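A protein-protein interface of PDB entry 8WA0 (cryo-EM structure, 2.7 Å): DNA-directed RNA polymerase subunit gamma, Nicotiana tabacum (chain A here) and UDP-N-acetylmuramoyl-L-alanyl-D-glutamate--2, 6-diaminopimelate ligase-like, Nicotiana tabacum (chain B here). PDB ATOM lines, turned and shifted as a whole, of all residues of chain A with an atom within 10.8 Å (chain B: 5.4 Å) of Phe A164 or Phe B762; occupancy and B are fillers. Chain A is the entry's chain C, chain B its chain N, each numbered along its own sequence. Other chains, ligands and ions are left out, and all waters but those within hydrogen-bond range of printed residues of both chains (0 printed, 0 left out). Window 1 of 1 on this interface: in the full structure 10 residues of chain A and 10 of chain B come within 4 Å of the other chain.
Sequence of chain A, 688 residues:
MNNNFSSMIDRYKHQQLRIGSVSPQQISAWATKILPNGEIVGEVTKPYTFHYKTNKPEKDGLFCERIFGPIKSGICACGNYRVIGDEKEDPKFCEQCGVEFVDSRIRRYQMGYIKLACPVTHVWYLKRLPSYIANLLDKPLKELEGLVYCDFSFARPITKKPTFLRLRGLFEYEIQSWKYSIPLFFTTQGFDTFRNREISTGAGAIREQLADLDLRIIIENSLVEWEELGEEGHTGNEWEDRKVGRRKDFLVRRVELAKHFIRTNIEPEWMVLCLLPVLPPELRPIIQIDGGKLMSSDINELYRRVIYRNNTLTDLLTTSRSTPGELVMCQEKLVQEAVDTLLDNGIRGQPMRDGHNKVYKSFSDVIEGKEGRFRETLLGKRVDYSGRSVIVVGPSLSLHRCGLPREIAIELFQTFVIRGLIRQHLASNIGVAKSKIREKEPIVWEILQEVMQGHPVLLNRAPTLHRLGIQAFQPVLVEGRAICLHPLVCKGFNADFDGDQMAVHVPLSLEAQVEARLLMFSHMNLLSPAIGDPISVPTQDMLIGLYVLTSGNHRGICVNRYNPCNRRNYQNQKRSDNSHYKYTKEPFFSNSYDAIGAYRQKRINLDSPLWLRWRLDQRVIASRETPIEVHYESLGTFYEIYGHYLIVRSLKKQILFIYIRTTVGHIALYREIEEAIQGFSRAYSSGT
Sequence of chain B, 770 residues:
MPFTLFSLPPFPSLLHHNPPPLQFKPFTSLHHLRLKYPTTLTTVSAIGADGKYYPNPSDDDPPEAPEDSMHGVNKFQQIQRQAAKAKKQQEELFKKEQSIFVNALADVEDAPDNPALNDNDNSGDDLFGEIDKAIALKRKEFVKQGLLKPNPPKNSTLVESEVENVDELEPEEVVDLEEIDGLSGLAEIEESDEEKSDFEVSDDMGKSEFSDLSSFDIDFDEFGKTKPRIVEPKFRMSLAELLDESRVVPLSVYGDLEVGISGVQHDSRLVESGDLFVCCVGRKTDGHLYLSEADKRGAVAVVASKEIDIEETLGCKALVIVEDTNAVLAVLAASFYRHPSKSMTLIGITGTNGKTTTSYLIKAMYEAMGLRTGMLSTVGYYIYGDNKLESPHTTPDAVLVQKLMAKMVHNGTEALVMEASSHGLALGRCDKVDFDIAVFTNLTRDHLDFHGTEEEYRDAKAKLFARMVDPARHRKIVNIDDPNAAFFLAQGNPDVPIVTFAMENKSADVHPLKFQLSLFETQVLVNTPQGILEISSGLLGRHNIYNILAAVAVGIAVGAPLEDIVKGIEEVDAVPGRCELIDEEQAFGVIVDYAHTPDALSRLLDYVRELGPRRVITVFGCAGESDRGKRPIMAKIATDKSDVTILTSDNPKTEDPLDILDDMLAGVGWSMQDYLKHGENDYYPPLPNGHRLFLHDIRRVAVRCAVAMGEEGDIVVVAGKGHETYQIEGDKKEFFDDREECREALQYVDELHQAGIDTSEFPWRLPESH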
ATOM      1  N   ALA A 155      -1.969  -6.790   2.447  1.00  0.00           N
ATOM      2  CA  ALA A 155      -1.388  -6.319   1.207  1.00  0.00           C
ATOM      3  C   ALA A 155       0.000  -6.870   1.008  1.00  0.00           C
ATOM      4  O   ALA A 155       0.434  -7.059  -0.126  1.00  0.00           O
ATOM      5  CB  ALA A 155      -1.362  -4.803   1.184  1.00  0.00           C
ATOM      6  N   ARG A 156       0.710  -7.116   2.102  1.00  0.00           N
ATOM      7  CA  ARG A 156       2.036  -7.727   1.983  1.00  0.00           C
ATOM      8  C   ARG A 156       2.131  -9.054   2.702  1.00  0.00           C
ATOM      9  O   ARG A 156       2.763  -9.156   3.748  1.00  0.00           O
ATOM     10  CB  ARG A 156       3.126  -6.759   2.457  1.00  0.00           C
ATOM     11  N   ILE A 158       3.733 -12.140   2.005  1.00  0.00           N
ATOM     12  CA  ILE A 158       4.972 -12.891   2.150  1.00  0.00           C
ATOM     13  C   ILE A 158       6.219 -12.042   2.052  1.00  0.00           C
ATOM     14  O   ILE A 158       6.406 -11.328   1.071  1.00  0.00           O
ATOM     15  CB  ILE A 158       5.098 -13.969   1.075  1.00  0.00           C
ATOM     16  N   LYS A 160       8.982 -13.534   2.154  1.00  0.00           N
ATOM     17  CA  LYS A 160       9.892 -14.485   1.537  1.00  0.00           C
ATOM     18  C   LYS A 160      10.325 -14.135   0.126  1.00  0.00           C
ATOM     19  O   LYS A 160      11.480 -14.345  -0.210  1.00  0.00           O
ATOM     20  CB  LYS A 160       9.275 -15.892   1.525  1.00  0.00           C
ATOM     21  N   LYS A 161       9.412 -13.643  -0.710  1.00  0.00           N
ATOM     22  CA  LYS A 161       9.755 -13.387  -2.116  1.00  0.00           C
ATOM     23  C   LYS A 161       9.499 -11.949  -2.608  1.00  0.00           C
ATOM     24  O   LYS A 161       8.539 -11.302  -2.190  1.00  0.00           O
ATOM     25  CB  LYS A 161       9.116 -14.419  -3.039  1.00  0.00           C
ATOM     26  N   PRO A 162      10.385 -11.441  -3.485  1.00  0.00           N
ATOM     27  CA  PRO A 162      10.243 -10.055  -3.937  1.00  0.00           C
ATOM     28  C   PRO A 162       8.985  -9.812  -4.774  1.00  0.00           C
ATOM     29  O   PRO A 162       8.585 -10.678  -5.547  1.00  0.00           O
ATOM     30  CB  PRO A 162      11.517  -9.828  -4.738  1.00  0.00           C
ATOM     31  N   THR A 163       8.358  -8.652  -4.603  1.00  0.00           N
ATOM     32  CA  THR A 163       7.148  -8.329  -5.346  1.00  0.00           C
ATOM     33  C   THR A 163       7.205  -6.940  -5.999  1.00  0.00           C
ATOM     34  O   THR A 163       7.616  -5.966  -5.361  1.00  0.00           O
ATOM     35  CB  THR A 163       5.916  -8.423  -4.448  1.00  0.00           C
ATOM     36  N   PHE A 164       6.777  -6.840  -7.265  1.00  0.00           N
ATOM     37  CA  PHE A 164       6.797  -5.561  -7.976  1.00  0.00           C
ATOM     38  C   PHE A 164       5.915  -4.468  -7.381  1.00  0.00           C
ATOM     39  O   PHE A 164       6.376  -3.366  -7.165  1.00  0.00           O
ATOM     40  CB  PHE A 164       6.369  -5.802  -9.414  1.00  0.00           C
ATOM     41  N   LEU A 165       4.674  -4.769  -7.045  1.00  0.00           N
ATOM     42  CA  LEU A 165       3.848  -3.763  -6.387  1.00  0.00           C
ATOM     43  C   LEU A 165       4.422  -3.456  -4.995  1.00  0.00           C
ATOM     44  O   LEU A 165       4.894  -4.365  -4.322  1.00  0.00           O
ATOM     45  CB  LEU A 165       2.408  -4.266  -6.282  1.00  0.00           C
ATOM     46  N   ARG A 166       4.416  -2.202  -4.557  1.00  0.00           N
ATOM     47  CA  ARG A 166       5.048  -1.908  -3.263  1.00  0.00           C
ATOM     48  C   ARG A 166       4.379  -1.047  -2.186  1.00  0.00           C
ATOM     49  O   ARG A 166       5.069  -0.270  -1.528  1.00  0.00           O
ATOM     50  CB  ARG A 166       6.467  -1.406  -3.454  1.00  0.00           C
ATOM     51  N   LEU A 167       3.077  -1.187  -1.990  1.00  0.00           N
ATOM     52  CA  LEU A 167       2.427  -0.455  -0.910  1.00  0.00           C
ATOM     53  C   LEU A 167       2.874  -1.031   0.423  1.00  0.00           C
ATOM     54  O   LEU A 167       2.979  -0.295   1.403  1.00  0.00           O
ATOM     55  CB  LEU A 167       0.906  -0.545  -1.030  1.00  0.00           C
ATOM     56  N   ARG A 168       3.114  -2.342   0.469  1.00  0.00           N
ATOM     57  CA  ARG A 168       3.544  -3.015   1.706  1.00  0.00           C
ATOM     58  C   ARG A 168       2.557  -2.766   2.824  1.00  0.00           C
ATOM     59  O   ARG A 168       2.948  -2.587   3.976  1.00  0.00           O
ATOM     60  CB  ARG A 168       4.968  -2.621   2.122  1.00  0.00           C
ATOM     61  N   PHE A 186      -2.038  -6.886 -16.868  1.00  0.00           N
ATOM     62  CA  PHE A 186      -1.312  -8.106 -16.587  1.00  0.00           C
ATOM     63  C   PHE A 186      -1.811  -9.267 -17.418  1.00  0.00           C
ATOM     64  O   PHE A 186      -2.920  -9.243 -17.937  1.00  0.00           O
ATOM     65  CB  PHE A 186      -1.399  -8.434 -15.100  1.00  0.00           C
ATOM     66  N   GLY A 190      -0.917 -13.676 -14.570  1.00  0.00           N
ATOM     67  CA  GLY A 190       0.257 -12.890 -14.239  1.00  0.00           C
ATOM     68  C   GLY A 190      -0.215 -12.187 -12.997  1.00  0.00           C
ATOM     69  O   GLY A 190       0.525 -12.035 -12.026  1.00  0.00           O
ATOM     70  N   PHE A 191      -1.476 -11.764 -13.026  1.00  0.00           N
ATOM     71  CA  PHE A 191      -2.060 -11.106 -11.879  1.00  0.00           C
ATOM     72  C   PHE A 191      -2.062 -12.081 -10.734  1.00  0.00           C
ATOM     73  O   PHE A 191      -1.834 -11.698  -9.604  1.00  0.00           O
ATOM     74  CB  PHE A 191      -3.489 -10.671 -12.184  1.00  0.00           C
ATOM     75  N   THR A 193       0.000 -14.505  -9.955  1.00  0.00           N
ATOM     76  CA  THR A 193       1.296 -14.590  -9.308  1.00  0.00           C
ATOM     77  C   THR A 193       1.548 -13.363  -8.458  1.00  0.00           C
ATOM     78  O   THR A 193       2.030 -13.469  -7.332  1.00  0.00           O
ATOM     79  CB  THR A 193       2.427 -14.703 -10.335  1.00  0.00           C
ATOM     80  N   PHE A 194       1.232 -12.193  -8.996  1.00  0.00           N
ATOM     81  CA  PHE A 194       1.383 -10.971  -8.227  1.00  0.00           C
ATOM     82  C   PHE A 194       0.437 -10.901  -7.033  1.00  0.00           C
ATOM     83  O   PHE A 194       0.839 -10.510  -5.942  1.00  0.00           O
ATOM     84  CB  PHE A 194       1.175  -9.764  -9.139  1.00  0.00           C
ATOM     85  N   ARG A 195      -0.816 -11.282  -7.235  1.00  0.00           N
ATOM     86  CA  ARG A 195      -1.804 -11.201  -6.164  1.00  0.00           C
ATOM     87  C   ARG A 195      -1.449 -12.129  -5.033  1.00  0.00           C
ATOM     88  O   ARG A 195      -1.576 -11.776  -3.872  1.00  0.00           O
ATOM     89  CB  ARG A 195      -3.205 -11.534  -6.684  1.00  0.00           C
ATOM     90  N   ASN A 196      -0.999 -13.327  -5.373  1.00  0.00           N
ATOM     91  CA  ASN A 196      -0.665 -14.286  -4.347  1.00  0.00           C
ATOM     92  C   ASN A 196       0.465 -13.706  -3.529  1.00  0.00           C
ATOM     93  O   ASN A 196       0.449 -13.776  -2.301  1.00  0.00           O
ATOM     94  CB  ASN A 196      -0.230 -15.599  -4.980  1.00  0.00           C
ATOM     95  N   ARG A 197       1.439 -13.107  -4.203  1.00  0.00           N
ATOM     96  CA  ARG A 197       2.554 -12.486  -3.501  1.00  0.00           C
ATOM     97  C   ARG A 197       2.086 -11.319  -2.654  1.00  0.00           C
ATOM     98  O   ARG A 197       2.593 -11.101  -1.554  1.00  0.00           O
ATOM     99  CB  ARG A 197       3.637 -12.046  -4.481  1.00  0.00           C
ATOM    100  N   GLU A 198       1.130 -10.553  -3.161  1.00  0.00           N
ATOM    101  CA  GLU A 198       0.705  -9.372  -2.437  1.00  0.00           C
ATOM    102  C   GLU A 198      -0.647  -9.466  -1.740  1.00  0.00           C
ATOM    103  O   GLU A 198      -0.703  -9.655  -0.528  1.00  0.00           O
ATOM    104  CB  GLU A 198       0.709  -8.173  -3.383  1.00  0.00           C
ATOM    105  N   ILE A 199      -1.741  -9.377  -2.487  1.00  0.00           N
ATOM    106  CA  ILE A 199      -3.055  -9.348  -1.842  1.00  0.00           C
ATOM    107  C   ILE A 199      -3.355 -10.609  -1.048  1.00  0.00           C
ATOM    108  O   ILE A 199      -3.081 -11.720  -1.500  1.00  0.00           O
ATOM    109  CB  ILE A 199      -4.181  -9.121  -2.863  1.00  0.00           C
ATOM    110  N   TYR B 675      19.221  -8.926  -0.394  1.00  0.00           N
ATOM    111  CA  TYR B 675      18.163  -8.250  -1.106  1.00  0.00           C
ATOM    112  C   TYR B 675      16.840  -8.418  -0.382  1.00  0.00           C
ATOM    113  O   TYR B 675      16.121  -7.447  -0.195  1.00  0.00           O
ATOM    114  CB  TYR B 675      18.049  -8.769  -2.536  1.00  0.00           C
ATOM    115  CG  TYR B 675      17.292  -7.837  -3.462  1.00  0.00           C
ATOM    116  CD1 TYR B 675      15.904  -7.793  -3.457  1.00  0.00           C
ATOM    117  CD2 TYR B 675      17.968  -7.001  -4.339  1.00  0.00           C
ATOM    118  CE1 TYR B 675      15.211  -6.941  -4.295  1.00  0.00           C
ATOM    119  CE2 TYR B 675      17.282  -6.148  -5.186  1.00  0.00           C
ATOM    120  CZ  TYR B 675      15.903  -6.124  -5.159  1.00  0.00           C
ATOM    121  OH  TYR B 675      15.211  -5.284  -5.998  1.00  0.00           O
ATOM    122  N   TYR B 684      16.290  -0.033  -0.897  1.00  0.00           N
ATOM    123  CA  TYR B 684      16.924  -0.720  -2.017  1.00  0.00           C
ATOM    124  C   TYR B 684      18.199   0.001  -2.442  1.00  0.00           C
ATOM    125  O   TYR B 684      18.205   0.699  -3.464  1.00  0.00           O
ATOM    126  CB  TYR B 684      15.959  -0.839  -3.198  1.00  0.00           C
ATOM    127  CG  TYR B 684      14.790  -1.762  -2.942  1.00  0.00           C
ATOM    128  CD1 TYR B 684      13.627  -1.296  -2.346  1.00  0.00           C
ATOM    129  CD2 TYR B 684      14.851  -3.103  -3.298  1.00  0.00           C
ATOM    130  CE1 TYR B 684      12.557  -2.137  -2.111  1.00  0.00           C
ATOM    131  CE2 TYR B 684      13.787  -3.953  -3.068  1.00  0.00           C
ATOM    132  CZ  TYR B 684      12.642  -3.465  -2.474  1.00  0.00           C
ATOM    133  OH  TYR B 684      11.578  -4.308  -2.241  1.00  0.00           O
ATOM    134  N   PHE B 694      17.640  -5.193 -10.258  1.00  0.00           N
ATOM    135  CA  PHE B 694      16.381  -5.750  -9.789  1.00  0.00           C
ATOM    136  C   PHE B 694      16.317  -7.230 -10.147  1.00  0.00           C
ATOM    137  O   PHE B 694      17.131  -7.743 -10.918  1.00  0.00           O
ATOM    138  CB  PHE B 694      15.183  -5.005 -10.392  1.00  0.00           C
ATOM    139  CG  PHE B 694      15.091  -3.564  -9.978  1.00  0.00           C
ATOM    140  CD1 PHE B 694      15.499  -3.164  -8.718  1.00  0.00           C
ATOM    141  CD2 PHE B 694      14.595  -2.610 -10.851  1.00  0.00           C
ATOM    142  CE1 PHE B 694      15.413  -1.838  -8.334  1.00  0.00           C
ATOM    143  CE2 PHE B 694      14.507  -1.283 -10.474  1.00  0.00           C
ATOM    144  CZ  PHE B 694      14.917  -0.898  -9.213  1.00  0.00           C
ATOM    145  N   LEU B 695      15.332  -7.918  -9.574  1.00  0.00           N
ATOM    146  CA  LEU B 695      15.142  -9.334  -9.852  1.00  0.00           C
ATOM    147  C   LEU B 695      13.715  -9.726  -9.501  1.00  0.00           C
ATOM    148  O   LEU B 695      13.079  -9.103  -8.646  1.00  0.00           O
ATOM    149  CB  LEU B 695      16.136 -10.210  -9.076  1.00  0.00           C
ATOM    150  CG  LEU B 695      15.812 -10.547  -7.617  1.00  0.00           C
ATOM    151  CD1 LEU B 695      16.734 -11.642  -7.103  1.00  0.00           C
ATOM    152  CD2 LEU B 695      15.904  -9.319  -6.728  1.00  0.00           C
ATOM    153  N   HIS B 696      13.223 -10.763 -10.174  1.00  0.00           N
ATOM    154  CA  HIS B 696      11.921 -11.334  -9.865  1.00  0.00           C
ATOM    155  C   HIS B 696      11.900 -12.778 -10.341  1.00  0.00           C
ATOM    156  O   HIS B 696      12.618 -13.152 -11.271  1.00  0.00           O
ATOM    157  CB  HIS B 696      10.779 -10.542 -10.508  1.00  0.00           C
ATOM    158  CG  HIS B 696       9.432 -10.853  -9.932  1.00  0.00           C
ATOM    159  ND1 HIS B 696       8.685 -11.941 -10.330  1.00  0.00           N
ATOM    160  CD2 HIS B 696       8.701 -10.221  -8.984  1.00  0.00           C
ATOM    161  CE1 HIS B 696       7.551 -11.965  -9.653  1.00  0.00           C
ATOM    162  NE2 HIS B 696       7.536 -10.932  -8.830  1.00  0.00           N
ATOM    163  N   VAL B 701       5.559 -11.084 -15.293  1.00  0.00           N
ATOM    164  CA  VAL B 701       5.373  -9.837 -14.555  1.00  0.00           C
ATOM    165  C   VAL B 701       6.627  -8.975 -14.636  1.00  0.00           C
ATOM    166  O   VAL B 701       6.547  -7.752 -14.810  1.00  0.00           O
ATOM    167  CB  VAL B 701       4.972 -10.136 -13.098  1.00  0.00           C
ATOM    168  CG1 VAL B 701       5.852 -11.226 -12.516  1.00  0.00           C
ATOM    169  CG2 VAL B 701       5.052  -8.876 -12.251  1.00  0.00           C
ATOM    170  N   CYS B 705       6.931  -5.317 -16.331  1.00  0.00           N
ATOM    171  CA  CYS B 705       7.438  -4.181 -15.570  1.00  0.00           C
ATOM    172  C   CYS B 705       8.599  -3.508 -16.291  1.00  0.00           C
ATOM    173  O   CYS B 705       8.665  -2.275 -16.354  1.00  0.00           O
ATOM    174  CB  CYS B 705       7.863  -4.634 -14.174  1.00  0.00           C
ATOM    175  N   SER B 760       8.516   3.837 -11.909  1.00  0.00           N
ATOM    176  CA  SER B 760       9.871   4.356 -12.061  1.00  0.00           C
ATOM    177  C   SER B 760      10.911   3.323 -11.646  1.00  0.00           C
ATOM    178  O   SER B 760      11.938   3.163 -12.316  1.00  0.00           O
ATOM    179  CB  SER B 760      10.035   5.642 -11.250  1.00  0.00           C
ATOM    180  OG  SER B 760       9.775   5.411  -9.876  1.00  0.00           O
ATOM    181  N   GLU B 761      10.663   2.612 -10.549  1.00  0.00           N
ATOM    182  CA  GLU B 761      11.580   1.607 -10.032  1.00  0.00           C
ATOM    183  C   GLU B 761      10.815   0.314  -9.774  1.00  0.00           C
ATOM    184  O   GLU B 761       9.625   0.195 -10.082  1.00  0.00           O
ATOM    185  CB  GLU B 761      12.277   2.096  -8.756  1.00  0.00           C
ATOM    186  N   PHE B 762      11.515  -0.666  -9.203  1.00  0.00           N
ATOM    187  CA  PHE B 762      10.884  -1.944  -8.882  1.00  0.00           C
ATOM    188  C   PHE B 762       9.812  -1.818  -7.806  1.00  0.00           C
ATOM    189  O   PHE B 762       8.724  -2.395  -7.981  1.00  0.00           O
ATOM    190  CB  PHE B 762      11.963  -2.961  -8.495  1.00  0.00           C
ATOM    191  CG  PHE B 762      11.483  -4.384  -8.481  1.00  0.00           C
ATOM    192  CD1 PHE B 762      11.251  -5.061  -9.668  1.00  0.00           C
ATOM    193  CD2 PHE B 762      11.281  -5.051  -7.285  1.00  0.00           C
ATOM    194  CE1 PHE B 762      10.816  -6.372  -9.661  1.00  0.00           C
ATOM    195  CE2 PHE B 762      10.847  -6.363  -7.271  1.00  0.00           C
ATOM    196  CZ  PHE B 762      10.613  -7.024  -8.461  1.00  0.00           C
ATOM    197  N   PRO B 763      10.027  -1.101  -6.683  1.00  0.00           N
ATOM    198  CA  PRO B 763       8.936  -0.942  -5.711  1.00  0.00           C
ATOM    199  C   PRO B 763       7.886   0.060  -6.167  1.00  0.00           C
ATOM    200  O   PRO B 763       7.960   1.244  -5.823  1.00  0.00           O
ATOM    201  CB  PRO B 763       9.661  -0.462  -4.448  1.00  0.00           C
ATOM    202  CG  PRO B 763      10.857   0.242  -4.958  1.00  0.00           C
ATOM    203  CD  PRO B 763      11.288  -0.524  -6.174  1.00  0.00           C
ATOM    204  N   TRP B 764       6.918  -0.403  -6.957  1.00  0.00           N
ATOM    205  CA  TRP B 764       5.852   0.468  -7.441  1.00  0.00           C
ATOM    206  C   TRP B 764       5.118   1.119  -6.277  1.00  0.00           C
ATOM    207  O   TRP B 764       4.664   0.439  -5.352  1.00  0.00           O
ATOM    208  CB  TRP B 764       4.863  -0.322  -8.300  1.00  0.00           C
ATOM    209  CG  TRP B 764       5.438  -0.886  -9.562  1.00  0.00           C
ATOM    210  CD1 TRP B 764       6.726  -0.783 -10.000  1.00  0.00           C
ATOM    211  CD2 TRP B 764       4.739  -1.646 -10.554  1.00  0.00           C
ATOM    212  NE1 TRP B 764       6.872  -1.430 -11.202  1.00  0.00           N
ATOM    213  CE2 TRP B 764       5.666  -1.969 -11.564  1.00  0.00           C
ATOM    214  CE3 TRP B 764       3.418  -2.085 -10.688  1.00  0.00           C
ATOM    215  CZ2 TRP B 764       5.315  -2.711 -12.692  1.00  0.00           C
ATOM    216  CZ3 TRP B 764       3.072  -2.820 -11.807  1.00  0.00           C
ATOM    217  CH2 TRP B 764       4.017  -3.126 -12.793  1.00  0.00           C
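NE2 of His B696 sits at hydrogen-bond distance from O of Pro A162 (3.5 Å). O of Phe B762 sits close to O of Phe A164 (2.7 Å). The backbone NH (N) of Trp B764 lies within hydrogen-bond range of the backbone carbonyl oxygen (O) of Phe A164. The backbone carbonyl oxygen of Trp B764 sits at hydrogen-bond distance from the backbone NH of Arg A166 (2.8 Å).
The backbone carbonyl oxygen (O) of Glu B761 sits close to the indole nitrogen (NE1) of Trp B764 (3.4 Å).
Among the printed residues, merely in contact across the chains: Arg A166 with Pro B763, Thr A163 with Phe B762, Phe A164 with Pro B763 and Leu A165 with Trp B764.
Phe A164 touches just these residues of chain B: Phe B762, Pro B763 and Trp B764. Phe B762 touches just these residues of chain A: Thr A163 and Phe A164. No residue of chain A comes within 4 Å of Phe B694. No residue of chain A comes within 4 Å of Glu B761. Pro B763 touches just these residues of chain A: Phe A164 and Arg A166. Of chain A, only Phe A164 (3.0 Å), Leu A165 (3.9 Å) and Arg A166 (2.8 Å) come within 4 Å of Trp B764. Of the printed residues of chain B, Pro A162 touches His B696 (3.5 Å). Of the printed residues of chain A, His B696 touches Pro A162 (3.5 Å). Of the printed residues of chain B, Leu A165 touches Trp B764 (3.9 Å). Printed residues of chain B within 4 Å of Thr A163: Phe B762 (3.8 Å). Arg A197 touches none of the printed residues of chain B. The nearest printed residue of chain B that does not touch Pro A162 is Leu B695 (4.3 Å).
Printed residues of chain A that touch a printed residue of chain B: Pro A162, Thr A163, Phe A164, Leu A165 and Arg A166. Of the 12 printed residues of chain B, 4 touch a printed residue of chain A. Hydrophobic or aromatic side chains of chain B within 4 Å of the printed part of chain A: His B696, Phe B762, Pro B763 and Trp B764. Among the printed residues, 8 pairs touch across the chains.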
